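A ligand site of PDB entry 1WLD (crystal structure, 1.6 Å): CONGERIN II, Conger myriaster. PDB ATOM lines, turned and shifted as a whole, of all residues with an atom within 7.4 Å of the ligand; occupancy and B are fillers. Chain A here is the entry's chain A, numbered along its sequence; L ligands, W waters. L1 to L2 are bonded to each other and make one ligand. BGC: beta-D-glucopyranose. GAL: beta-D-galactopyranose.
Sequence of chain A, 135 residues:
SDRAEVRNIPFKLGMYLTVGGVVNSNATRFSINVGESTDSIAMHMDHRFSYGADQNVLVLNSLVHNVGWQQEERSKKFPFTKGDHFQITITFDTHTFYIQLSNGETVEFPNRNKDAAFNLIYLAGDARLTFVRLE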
ATOM      1  N   ARG A  29      -3.706 -13.614   9.990  1.00  0.00           N
ATOM      2  CA  ARG A  29      -4.280 -14.569  10.908  1.00  0.00           C
ATOM      3  C   ARG A  29      -3.682 -14.385  12.312  1.00  0.00           C
ATOM      4  O   ARG A  29      -2.531 -13.928  12.411  1.00  0.00           O
ATOM      5  CB  ARG A  29      -4.021 -16.022  10.398  1.00  0.00           C
ATOM      6  CG  ARG A  29      -2.528 -16.242  10.175  1.00  0.00           C
ATOM      7  CD  ARG A  29      -2.137 -17.468   9.382  1.00  0.00           C
ATOM      8  NE  ARG A  29      -2.366 -18.678  10.138  1.00  0.00           N
ATOM      9  CZ  ARG A  29      -1.524 -19.634  10.479  1.00  0.00           C
ATOM     10  NH1 ARG A  29      -0.234 -19.707  10.211  1.00  0.00           N
ATOM     11  NH2 ARG A  29      -2.014 -20.652  11.185  1.00  0.00           N
ATOM     12  N   SER A  31      -3.971 -16.618  16.355  1.00  0.00           N
ATOM     13  CA  SER A  31      -4.654 -17.752  17.026  1.00  0.00           C
ATOM     14  C   SER A  31      -4.683 -17.555  18.536  1.00  0.00           C
ATOM     15  O   SER A  31      -3.821 -16.855  19.075  1.00  0.00           O
ATOM     16  CB  SER A  31      -3.920 -19.060  16.671  1.00  0.00           C
ATOM     17  OG  SER A  31      -2.569 -19.005  17.133  1.00  0.00           O
ATOM     18  N   ASN A  33      -4.572 -20.104  21.904  1.00  0.00           N
ATOM     19  CA  ASN A  33      -4.096 -21.477  22.077  1.00  0.00           C
ATOM     20  C   ASN A  33      -4.133 -21.894  23.547  1.00  0.00           C
ATOM     21  O   ASN A  33      -3.701 -21.098  24.380  1.00  0.00           O
ATOM     22  CB  ASN A  33      -2.618 -21.597  21.631  1.00  0.00           C
ATOM     23  CG  ASN A  33      -2.459 -21.204  20.172  1.00  0.00           C
ATOM     24  OD1 ASN A  33      -2.619 -22.063  19.301  1.00  0.00           O
ATOM     25  ND2 ASN A  33      -2.201 -19.919  19.888  1.00  0.00           N
ATOM     26  N   HIS A  44      -6.344 -25.107  19.608  1.00  0.00           N
ATOM     27  CA  HIS A  44      -5.878 -24.014  18.787  1.00  0.00           C
ATOM     28  C   HIS A  44      -7.033 -23.451  17.985  1.00  0.00           C
ATOM     29  O   HIS A  44      -7.684 -24.230  17.274  1.00  0.00           O
ATOM     30  CB  HIS A  44      -4.799 -24.519  17.834  1.00  0.00           C
ATOM     31  CG  HIS A  44      -4.378 -23.698  16.680  1.00  0.00           C
ATOM     32  ND1 HIS A  44      -3.490 -22.647  16.788  1.00  0.00           N
ATOM     33  CD2 HIS A  44      -4.685 -23.802  15.353  1.00  0.00           C
ATOM     34  CE1 HIS A  44      -3.263 -22.154  15.577  1.00  0.00           C
ATOM     35  NE2 HIS A  44      -3.982 -22.811  14.698  1.00  0.00           N
ATOM     36  N   MET A  45      -7.283 -22.156  18.097  1.00  0.00           N
ATOM     37  CA  MET A  45      -8.351 -21.544  17.297  1.00  0.00           C
ATOM     38  C   MET A  45      -7.736 -20.423  16.468  1.00  0.00           C
ATOM     39  O   MET A  45      -7.320 -19.403  17.024  1.00  0.00           O
ATOM     40  CB  MET A  45      -9.478 -20.975  18.166  1.00  0.00           C
ATOM     41  CG  MET A  45     -10.552 -20.350  17.248  1.00  0.00           C
ATOM     42  SD  MET A  45     -12.131 -19.970  18.048  1.00  0.00           S
ATOM     43  CE  MET A  45     -11.406 -19.028  19.425  1.00  0.00           C
ATOM     44  N   ASP A  46      -7.669 -20.622  15.153  1.00  0.00           N
ATOM     45  CA  ASP A  46      -6.991 -19.699  14.271  1.00  0.00           C
ATOM     46  C   ASP A  46      -8.040 -18.823  13.582  1.00  0.00           C
ATOM     47  O   ASP A  46      -9.050 -19.345  13.102  1.00  0.00           O
ATOM     48  CB  ASP A  46      -6.143 -20.488  13.245  1.00  0.00           C
ATOM     49  CG  ASP A  46      -5.097 -19.659  12.555  1.00  0.00           C
ATOM     50  OD1 ASP A  46      -4.717 -18.582  13.087  1.00  0.00           O
ATOM     51  OD2 ASP A  46      -4.674 -20.045  11.439  1.00  0.00           O
ATOM     52  N   ARG A  48      -8.556 -16.627  10.512  1.00  0.00           N
ATOM     53  CA  ARG A  48      -7.892 -16.430   9.239  1.00  0.00           C
ATOM     54  C   ARG A  48      -8.582 -15.355   8.398  1.00  0.00           C
ATOM     55  O   ARG A  48      -9.691 -15.586   7.940  1.00  0.00           O
ATOM     56  CB  ARG A  48      -7.832 -17.769   8.484  1.00  0.00           C
ATOM     57  CG  ARG A  48      -6.983 -18.793   9.261  1.00  0.00           C
ATOM     58  CD  ARG A  48      -6.978 -20.150   8.547  1.00  0.00           C
ATOM     59  NE  ARG A  48      -6.101 -21.073   9.305  1.00  0.00           N
ATOM     60  CZ  ARG A  48      -5.707 -22.267   8.908  1.00  0.00           C
ATOM     61  NH1 ARG A  48      -6.143 -22.674   7.701  1.00  0.00           N
ATOM     62  NH2 ARG A  48      -4.913 -23.031   9.637  1.00  0.00           N
ATOM     63  N   TYR A  51      -5.385 -16.473   4.437  1.00  0.00           N
ATOM     64  CA  TYR A  51      -4.355 -17.507   4.630  1.00  0.00           C
ATOM     65  C   TYR A  51      -4.578 -18.620   3.603  1.00  0.00           C
ATOM     66  O   TYR A  51      -5.509 -19.419   3.710  1.00  0.00           O
ATOM     67  CB  TYR A  51      -4.392 -18.069   6.039  1.00  0.00           C
ATOM     68  CG  TYR A  51      -3.368 -19.136   6.354  1.00  0.00           C
ATOM     69  CD1 TYR A  51      -2.025 -18.834   6.345  1.00  0.00           C
ATOM     70  CD2 TYR A  51      -3.745 -20.447   6.616  1.00  0.00           C
ATOM     71  CE1 TYR A  51      -1.053 -19.784   6.625  1.00  0.00           C
ATOM     72  CE2 TYR A  51      -2.795 -21.426   6.885  1.00  0.00           C
ATOM     73  CZ  TYR A  51      -1.457 -21.074   6.902  1.00  0.00           C
ATOM     74  OH  TYR A  51      -0.503 -22.041   7.150  1.00  0.00           O
ATOM     75  N   ALA A  53      -6.097 -20.389   0.875  1.00  0.00           N
ATOM     76  CA  ALA A  53      -7.446 -20.344   0.346  1.00  0.00           C
ATOM     77  C   ALA A  53      -8.504 -19.946   1.371  1.00  0.00           C
ATOM     78  O   ALA A  53      -9.682 -19.798   1.046  1.00  0.00           O
ATOM     79  CB  ALA A  53      -7.846 -21.739  -0.166  1.00  0.00           C
ATOM     80  N   ASP A  54      -8.102 -19.823   2.637  1.00  0.00           N
ATOM     81  CA  ASP A  54      -9.005 -19.458   3.709  1.00  0.00           C
ATOM     82  C   ASP A  54      -9.128 -17.946   3.862  1.00  0.00           C
ATOM     83  O   ASP A  54      -8.150 -17.258   4.143  1.00  0.00           O
ATOM     84  CB  ASP A  54      -8.490 -20.031   5.041  1.00  0.00           C
ATOM     85  CG  ASP A  54      -8.553 -21.546   5.053  1.00  0.00           C
ATOM     86  OD1 ASP A  54      -9.536 -22.075   4.499  1.00  0.00           O
ATOM     87  OD2 ASP A  54      -7.675 -22.218   5.623  1.00  0.00           O
ATOM     88  N   VAL A  59     -10.413 -21.754  12.061  1.00  0.00           N
ATOM     89  CA  VAL A  59      -9.920 -23.132  11.913  1.00  0.00           C
ATOM     90  C   VAL A  59      -9.436 -23.623  13.279  1.00  0.00           C
ATOM     91  O   VAL A  59      -8.598 -22.917  13.878  1.00  0.00           O
ATOM     92  CB  VAL A  59      -8.775 -23.223  10.888  1.00  0.00           C
ATOM     93  CG1 VAL A  59      -8.281 -24.653  10.793  1.00  0.00           C
ATOM     94  CG2 VAL A  59      -9.273 -22.757   9.506  1.00  0.00           C
ATOM     95  N   LEU A  60     -10.007 -24.697  13.769  1.00  0.00           N
ATOM     96  CA  LEU A  60      -9.644 -25.217  15.091  1.00  0.00           C
ATOM     97  C   LEU A  60      -8.943 -26.566  14.990  1.00  0.00           C
ATOM     98  O   LEU A  60      -9.264 -27.425  14.130  1.00  0.00           O
ATOM     99  CB  LEU A  60     -10.902 -25.380  15.949  1.00  0.00           C
ATOM    100  CG  LEU A  60     -11.624 -24.069  16.270  1.00  0.00           C
ATOM    101  CD1 LEU A  60     -12.658 -23.740  15.189  1.00  0.00           C
ATOM    102  CD2 LEU A  60     -12.314 -24.186  17.616  1.00  0.00           C
ATOM    103  N   ASN A  61      -7.983 -26.820  15.881  1.00  0.00           N
ATOM    104  CA  ASN A  61      -7.256 -28.111  15.798  1.00  0.00           C
ATOM    105  C   ASN A  61      -6.481 -28.315  17.090  1.00  0.00           C
ATOM    106  O   ASN A  61      -6.521 -27.460  17.958  1.00  0.00           O
ATOM    107  CB  ASN A  61      -6.332 -28.118  14.582  1.00  0.00           C
ATOM    108  CG  ASN A  61      -6.019 -29.523  14.068  1.00  0.00           C
ATOM    109  OD1 ASN A  61      -6.348 -30.494  14.761  1.00  0.00           O
ATOM    110  ND2 ASN A  61      -5.424 -29.642  12.877  1.00  0.00           N
ATOM    111  N   SER A  62      -5.880 -29.485  17.224  1.00  0.00           N
ATOM    112  CA  SER A  62      -4.955 -29.777  18.318  1.00  0.00           C
ATOM    113  C   SER A  62      -3.584 -30.093  17.735  1.00  0.00           C
ATOM    114  O   SER A  62      -3.460 -30.589  16.613  1.00  0.00           O
ATOM    115  CB  SER A  62      -5.454 -30.934  19.192  1.00  0.00           C
ATOM    116  OG  SER A  62      -5.760 -32.049  18.351  1.00  0.00           O
ATOM    117  N   TRP A  69      -0.197 -31.622  13.680  1.00  0.00           N
ATOM    118  CA  TRP A  69      -1.587 -31.217  13.709  1.00  0.00           C
ATOM    119  C   TRP A  69      -2.492 -32.408  13.421  1.00  0.00           C
ATOM    120  O   TRP A  69      -2.161 -33.287  12.598  1.00  0.00           O
ATOM    121  CB  TRP A  69      -1.828 -30.091  12.710  1.00  0.00           C
ATOM    122  CG  TRP A  69      -1.108 -28.834  13.124  1.00  0.00           C
ATOM    123  CD1 TRP A  69       0.052 -28.334  12.640  1.00  0.00           C
ATOM    124  CD2 TRP A  69      -1.531 -27.932  14.174  1.00  0.00           C
ATOM    125  NE1 TRP A  69       0.397 -27.176  13.285  1.00  0.00           N
ATOM    126  CE2 TRP A  69      -0.563 -26.920  14.234  1.00  0.00           C
ATOM    127  CE3 TRP A  69      -2.613 -27.874  15.032  1.00  0.00           C
ATOM    128  CZ2 TRP A  69      -0.656 -25.838  15.134  1.00  0.00           C
ATOM    129  CZ3 TRP A  69      -2.704 -26.825  15.948  1.00  0.00           C
ATOM    130  CH2 TRP A  69      -1.729 -25.826  15.973  1.00  0.00           C
ATOM    131  N   GLN A  70      -3.581 -32.460  14.166  1.00  0.00           N
ATOM    132  CA  GLN A  70      -4.585 -33.511  14.021  1.00  0.00           C
ATOM    133  C   GLN A  70      -5.671 -33.093  13.021  1.00  0.00           C
ATOM    134  O   GLN A  70      -5.361 -32.375  12.072  1.00  0.00           O
ATOM    135  CB  GLN A  70      -5.100 -33.880  15.408  1.00  0.00           C
ATOM    136  CG  GLN A  70      -3.945 -34.320  16.358  1.00  0.00           C
ATOM    137  CD  GLN A  70      -3.140 -35.452  15.731  1.00  0.00           C
ATOM    138  OE1 GLN A  70      -3.723 -36.492  15.452  1.00  0.00           O
ATOM    139  NE2 GLN A  70      -1.847 -35.295  15.499  1.00  0.00           N
ATOM    140  N   GLN A  71      -6.896 -33.531  13.267  1.00  0.00           N
ATOM    141  CA  GLN A  71      -7.971 -33.283  12.303  1.00  0.00           C
ATOM    142  C   GLN A  71      -8.555 -31.882  12.526  1.00  0.00           C
ATOM    143  O   GLN A  71      -9.114 -31.612  13.590  1.00  0.00           O
ATOM    144  CB  GLN A  71      -9.052 -34.342  12.431  1.00  0.00           C
ATOM    145  CG  GLN A  71     -10.342 -34.034  11.690  1.00  0.00           C
ATOM    146  CD  GLN A  71     -10.151 -34.093  10.193  1.00  0.00           C
ATOM    147  OE1 GLN A  71      -9.838 -35.179   9.669  1.00  0.00           O
ATOM    148  NE2 GLN A  71     -10.342 -32.965   9.507  1.00  0.00           N
ATOM    149  N   GLU A  72      -8.469 -31.052  11.486  1.00  0.00           N
ATOM    150  CA  GLU A  72      -9.047 -29.716  11.590  1.00  0.00           C
ATOM    151  C   GLU A  72     -10.576 -29.715  11.611  1.00  0.00           C
ATOM    152  O   GLU A  72     -11.225 -30.489  10.922  1.00  0.00           O
ATOM    153  CB  GLU A  72      -8.695 -28.855  10.364  1.00  0.00           C
ATOM    154  CG  GLU A  72      -7.257 -28.437  10.290  1.00  0.00           C
ATOM    155  CD  GLU A  72      -6.992 -27.517   9.117  1.00  0.00           C
ATOM    156  OE1 GLU A  72      -7.856 -27.297   8.218  1.00  0.00           O
ATOM    157  OE2 GLU A  72      -5.855 -27.051   9.105  1.00  0.00           O
ATOM    158  N   GLU A  73     -11.120 -28.744  12.324  1.00  0.00           N
ATOM    159  CA  GLU A  73     -12.536 -28.389  12.306  1.00  0.00           C
ATOM    160  C   GLU A  73     -12.618 -26.936  11.863  1.00  0.00           C
ATOM    161  O   GLU A  73     -11.709 -26.131  12.105  1.00  0.00           O
ATOM    162  CB  GLU A  73     -13.179 -28.603  13.678  1.00  0.00           C
ATOM    163  CG  GLU A  73     -13.187 -30.061  14.097  1.00  0.00           C
ATOM    164  CD  GLU A  73     -14.087 -30.433  15.228  1.00  0.00           C
ATOM    165  OE1 GLU A  73     -14.216 -31.658  15.485  1.00  0.00           O
ATOM    166  OE2 GLU A  73     -14.711 -29.617  15.930  1.00  0.00           O
ATOM    167  N   ARG A  74     -13.635 -26.594  11.081  1.00  0.00           N
ATOM    168  CA  ARG A  74     -13.772 -25.218  10.622  1.00  0.00           C
ATOM    169  C   ARG A  74     -15.117 -24.623  11.014  1.00  0.00           C
ATOM    170  O   ARG A  74     -16.104 -25.320  11.222  1.00  0.00           O
ATOM    171  CB  ARG A  74     -13.598 -25.196   9.090  1.00  0.00           C
ATOM    172  CG  ARG A  74     -12.147 -25.488   8.753  1.00  0.00           C
ATOM    173  CD  ARG A  74     -11.830 -25.566   7.275  1.00  0.00           C
ATOM    174  NE  ARG A  74     -10.344 -25.708   7.177  1.00  0.00           N
ATOM    175  CZ  ARG A  74      -9.671 -24.855   6.412  1.00  0.00           C
ATOM    176  NH1 ARG A  74     -10.390 -23.949   5.780  1.00  0.00           N
ATOM    177  NH2 ARG A  74      -8.351 -24.952   6.316  1.00  0.00           N
HETATM  178  C2  BGC L   1      -4.518 -26.841   5.657  1.00  0.00           C
HETATM  179  C3  BGC L   1      -4.092 -25.723   6.608  1.00  0.00           C
HETATM  180  C4  BGC L   1      -2.850 -26.144   7.387  1.00  0.00           C
HETATM  181  C5  BGC L   1      -1.777 -26.554   6.373  1.00  0.00           C
HETATM  182  C6  BGC L   1      -0.510 -27.037   6.971  1.00  0.00           C
HETATM  183  C1  BGC L   1      -3.360 -27.162   4.750  1.00  0.00           C
HETATM  184  O1  BGC L   1      -3.953 -28.495   4.082  1.00  0.00           O
HETATM  185  O2  BGC L   1      -5.608 -26.351   4.884  1.00  0.00           O
HETATM  186  O3  BGC L   1      -5.151 -25.404   7.463  1.00  0.00           O
HETATM  187  O4  BGC L   1      -2.361 -25.026   8.077  1.00  0.00           O
HETATM  188  O5  BGC L   1      -2.309 -27.659   5.572  1.00  0.00           O
HETATM  189  O6  BGC L   1      -0.680 -28.027   7.991  1.00  0.00           O
HETATM  190  C1  GAL L   2      -2.054 -25.247   9.443  1.00  0.00           C
HETATM  191  C2  GAL L   2      -1.375 -23.968   9.943  1.00  0.00           C
HETATM  192  C3  GAL L   2      -1.123 -24.119  11.288  1.00  0.00           C
HETATM  193  C4  GAL L   2      -2.422 -24.355  12.170  1.00  0.00           C
HETATM  194  C5  GAL L   2      -3.076 -25.589  11.544  1.00  0.00           C
HETATM  195  C6  GAL L   2      -4.443 -25.910  12.120  1.00  0.00           C
HETATM  196  O2  GAL L   2      -0.135 -23.824   9.268  1.00  0.00           O
HETATM  197  O3  GAL L   2      -0.413 -22.971  11.906  1.00  0.00           O
HETATM  198  O4  GAL L   2      -3.256 -23.203  12.084  1.00  0.00           O
HETATM  199  O5  GAL L   2      -3.297 -25.390  10.131  1.00  0.00           O
HETATM  200  O6  GAL L   2      -4.847 -27.187  11.596  1.00  0.00           O
HETATM  201  O   HOH W   1      -3.517 -29.120   9.669  1.00  0.00           O
HETATM  202  O   HOH W   2      -4.320 -30.727   5.758  1.00  0.00           O
HETATM  203  O   HOH W   3       1.876 -21.514  10.491  1.00  0.00           O
HETATM  204  O   HOH W   4       2.274 -25.235   9.285  1.00  0.00           O
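OE2 of Glu 72 lies within hydrogen-bond range of O3 of BGC L1, 2.4 Å away.
A ring nitrogen (NE2) of His 44 sits at hydrogen-bond distance from an oxygen (O4) of GAL L2, 2.7 Å away.
The side-chain hydroxyl (OH) of Tyr 51 is in hydrogen-bond range of an oxygen (O2) of GAL L2.
The side-chain amide nitrogen (ND2) of Asn 61 sits at hydrogen-bond distance from an oxygen (O6) of GAL L2 (2.8 Å).
The guanidinium group (NH2) of Arg 48 is in hydrogen-bond range of an oxygen (O5) of GAL L2 (2.9 Å).
An oxygen (O3) of GAL L2 lies within hydrogen-bond range of the guanidinium group of Arg 29 (2.9 Å).
An oxygen (O2) of BGC L1 is in hydrogen-bond range of the guanidinium group (NH2) of Arg 74 (3.4 Å).
The side-chain carboxylate of Glu 72 lies within salt-bridge range of the guanidinium group of Arg 74 (3.1 Å).
The backbone carbonyl oxygen (O) of Asn 61 sits at hydrogen-bond distance from the backbone NH (N) of His 44 (2.9 Å).
A ring nitrogen (ND1) of His 44 is in hydrogen-bond range of the side-chain amide oxygen of Asn 33 (2.7 Å).
The backbone carbonyl oxygen of Gln 70 is in hydrogen-bond range of the side-chain amide nitrogen of Asn 61 (2.8 Å).
OD1 of Asn 61 lies close to O of Gln 71.
NE of Arg 48 lies within salt-bridge range of OD2 of Asp 46 (2.8 Å).
The guanidinium group of Arg 48 is in salt-bridge range of the side-chain carboxylate of Asp 54, 2.6 Å away.
The side-chain carboxylate (OD1) of Asp 54 lies within salt-bridge range of the guanidinium group (NH1) of Arg 74, at 2.4 Å.
Residues that only touch the ligand: Asp 46 (3.5 Å) and Trp 69 (3.8 Å).
Hydrophobic or aromatic side chains within 4 Å of the ligand: His 44, Tyr 51 and Trp 69.
Nine residues have an atom within 4 Å of the ligand: Arg 29, His 44, Asp 46, Arg 48, Tyr 51, Asn 61, Trp 69, Glu 72 and Arg 74.
Water W1 bridges an oxygen (O6) of GAL L2 (3.0 Å) and the side-chain carboxylate of Glu 72 (3.2 Å).
Water W3 lies within hydrogen-bond range of NH1 of Arg 29 (2.8 Å) and O3 of GAL L2 (3.1 Å).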
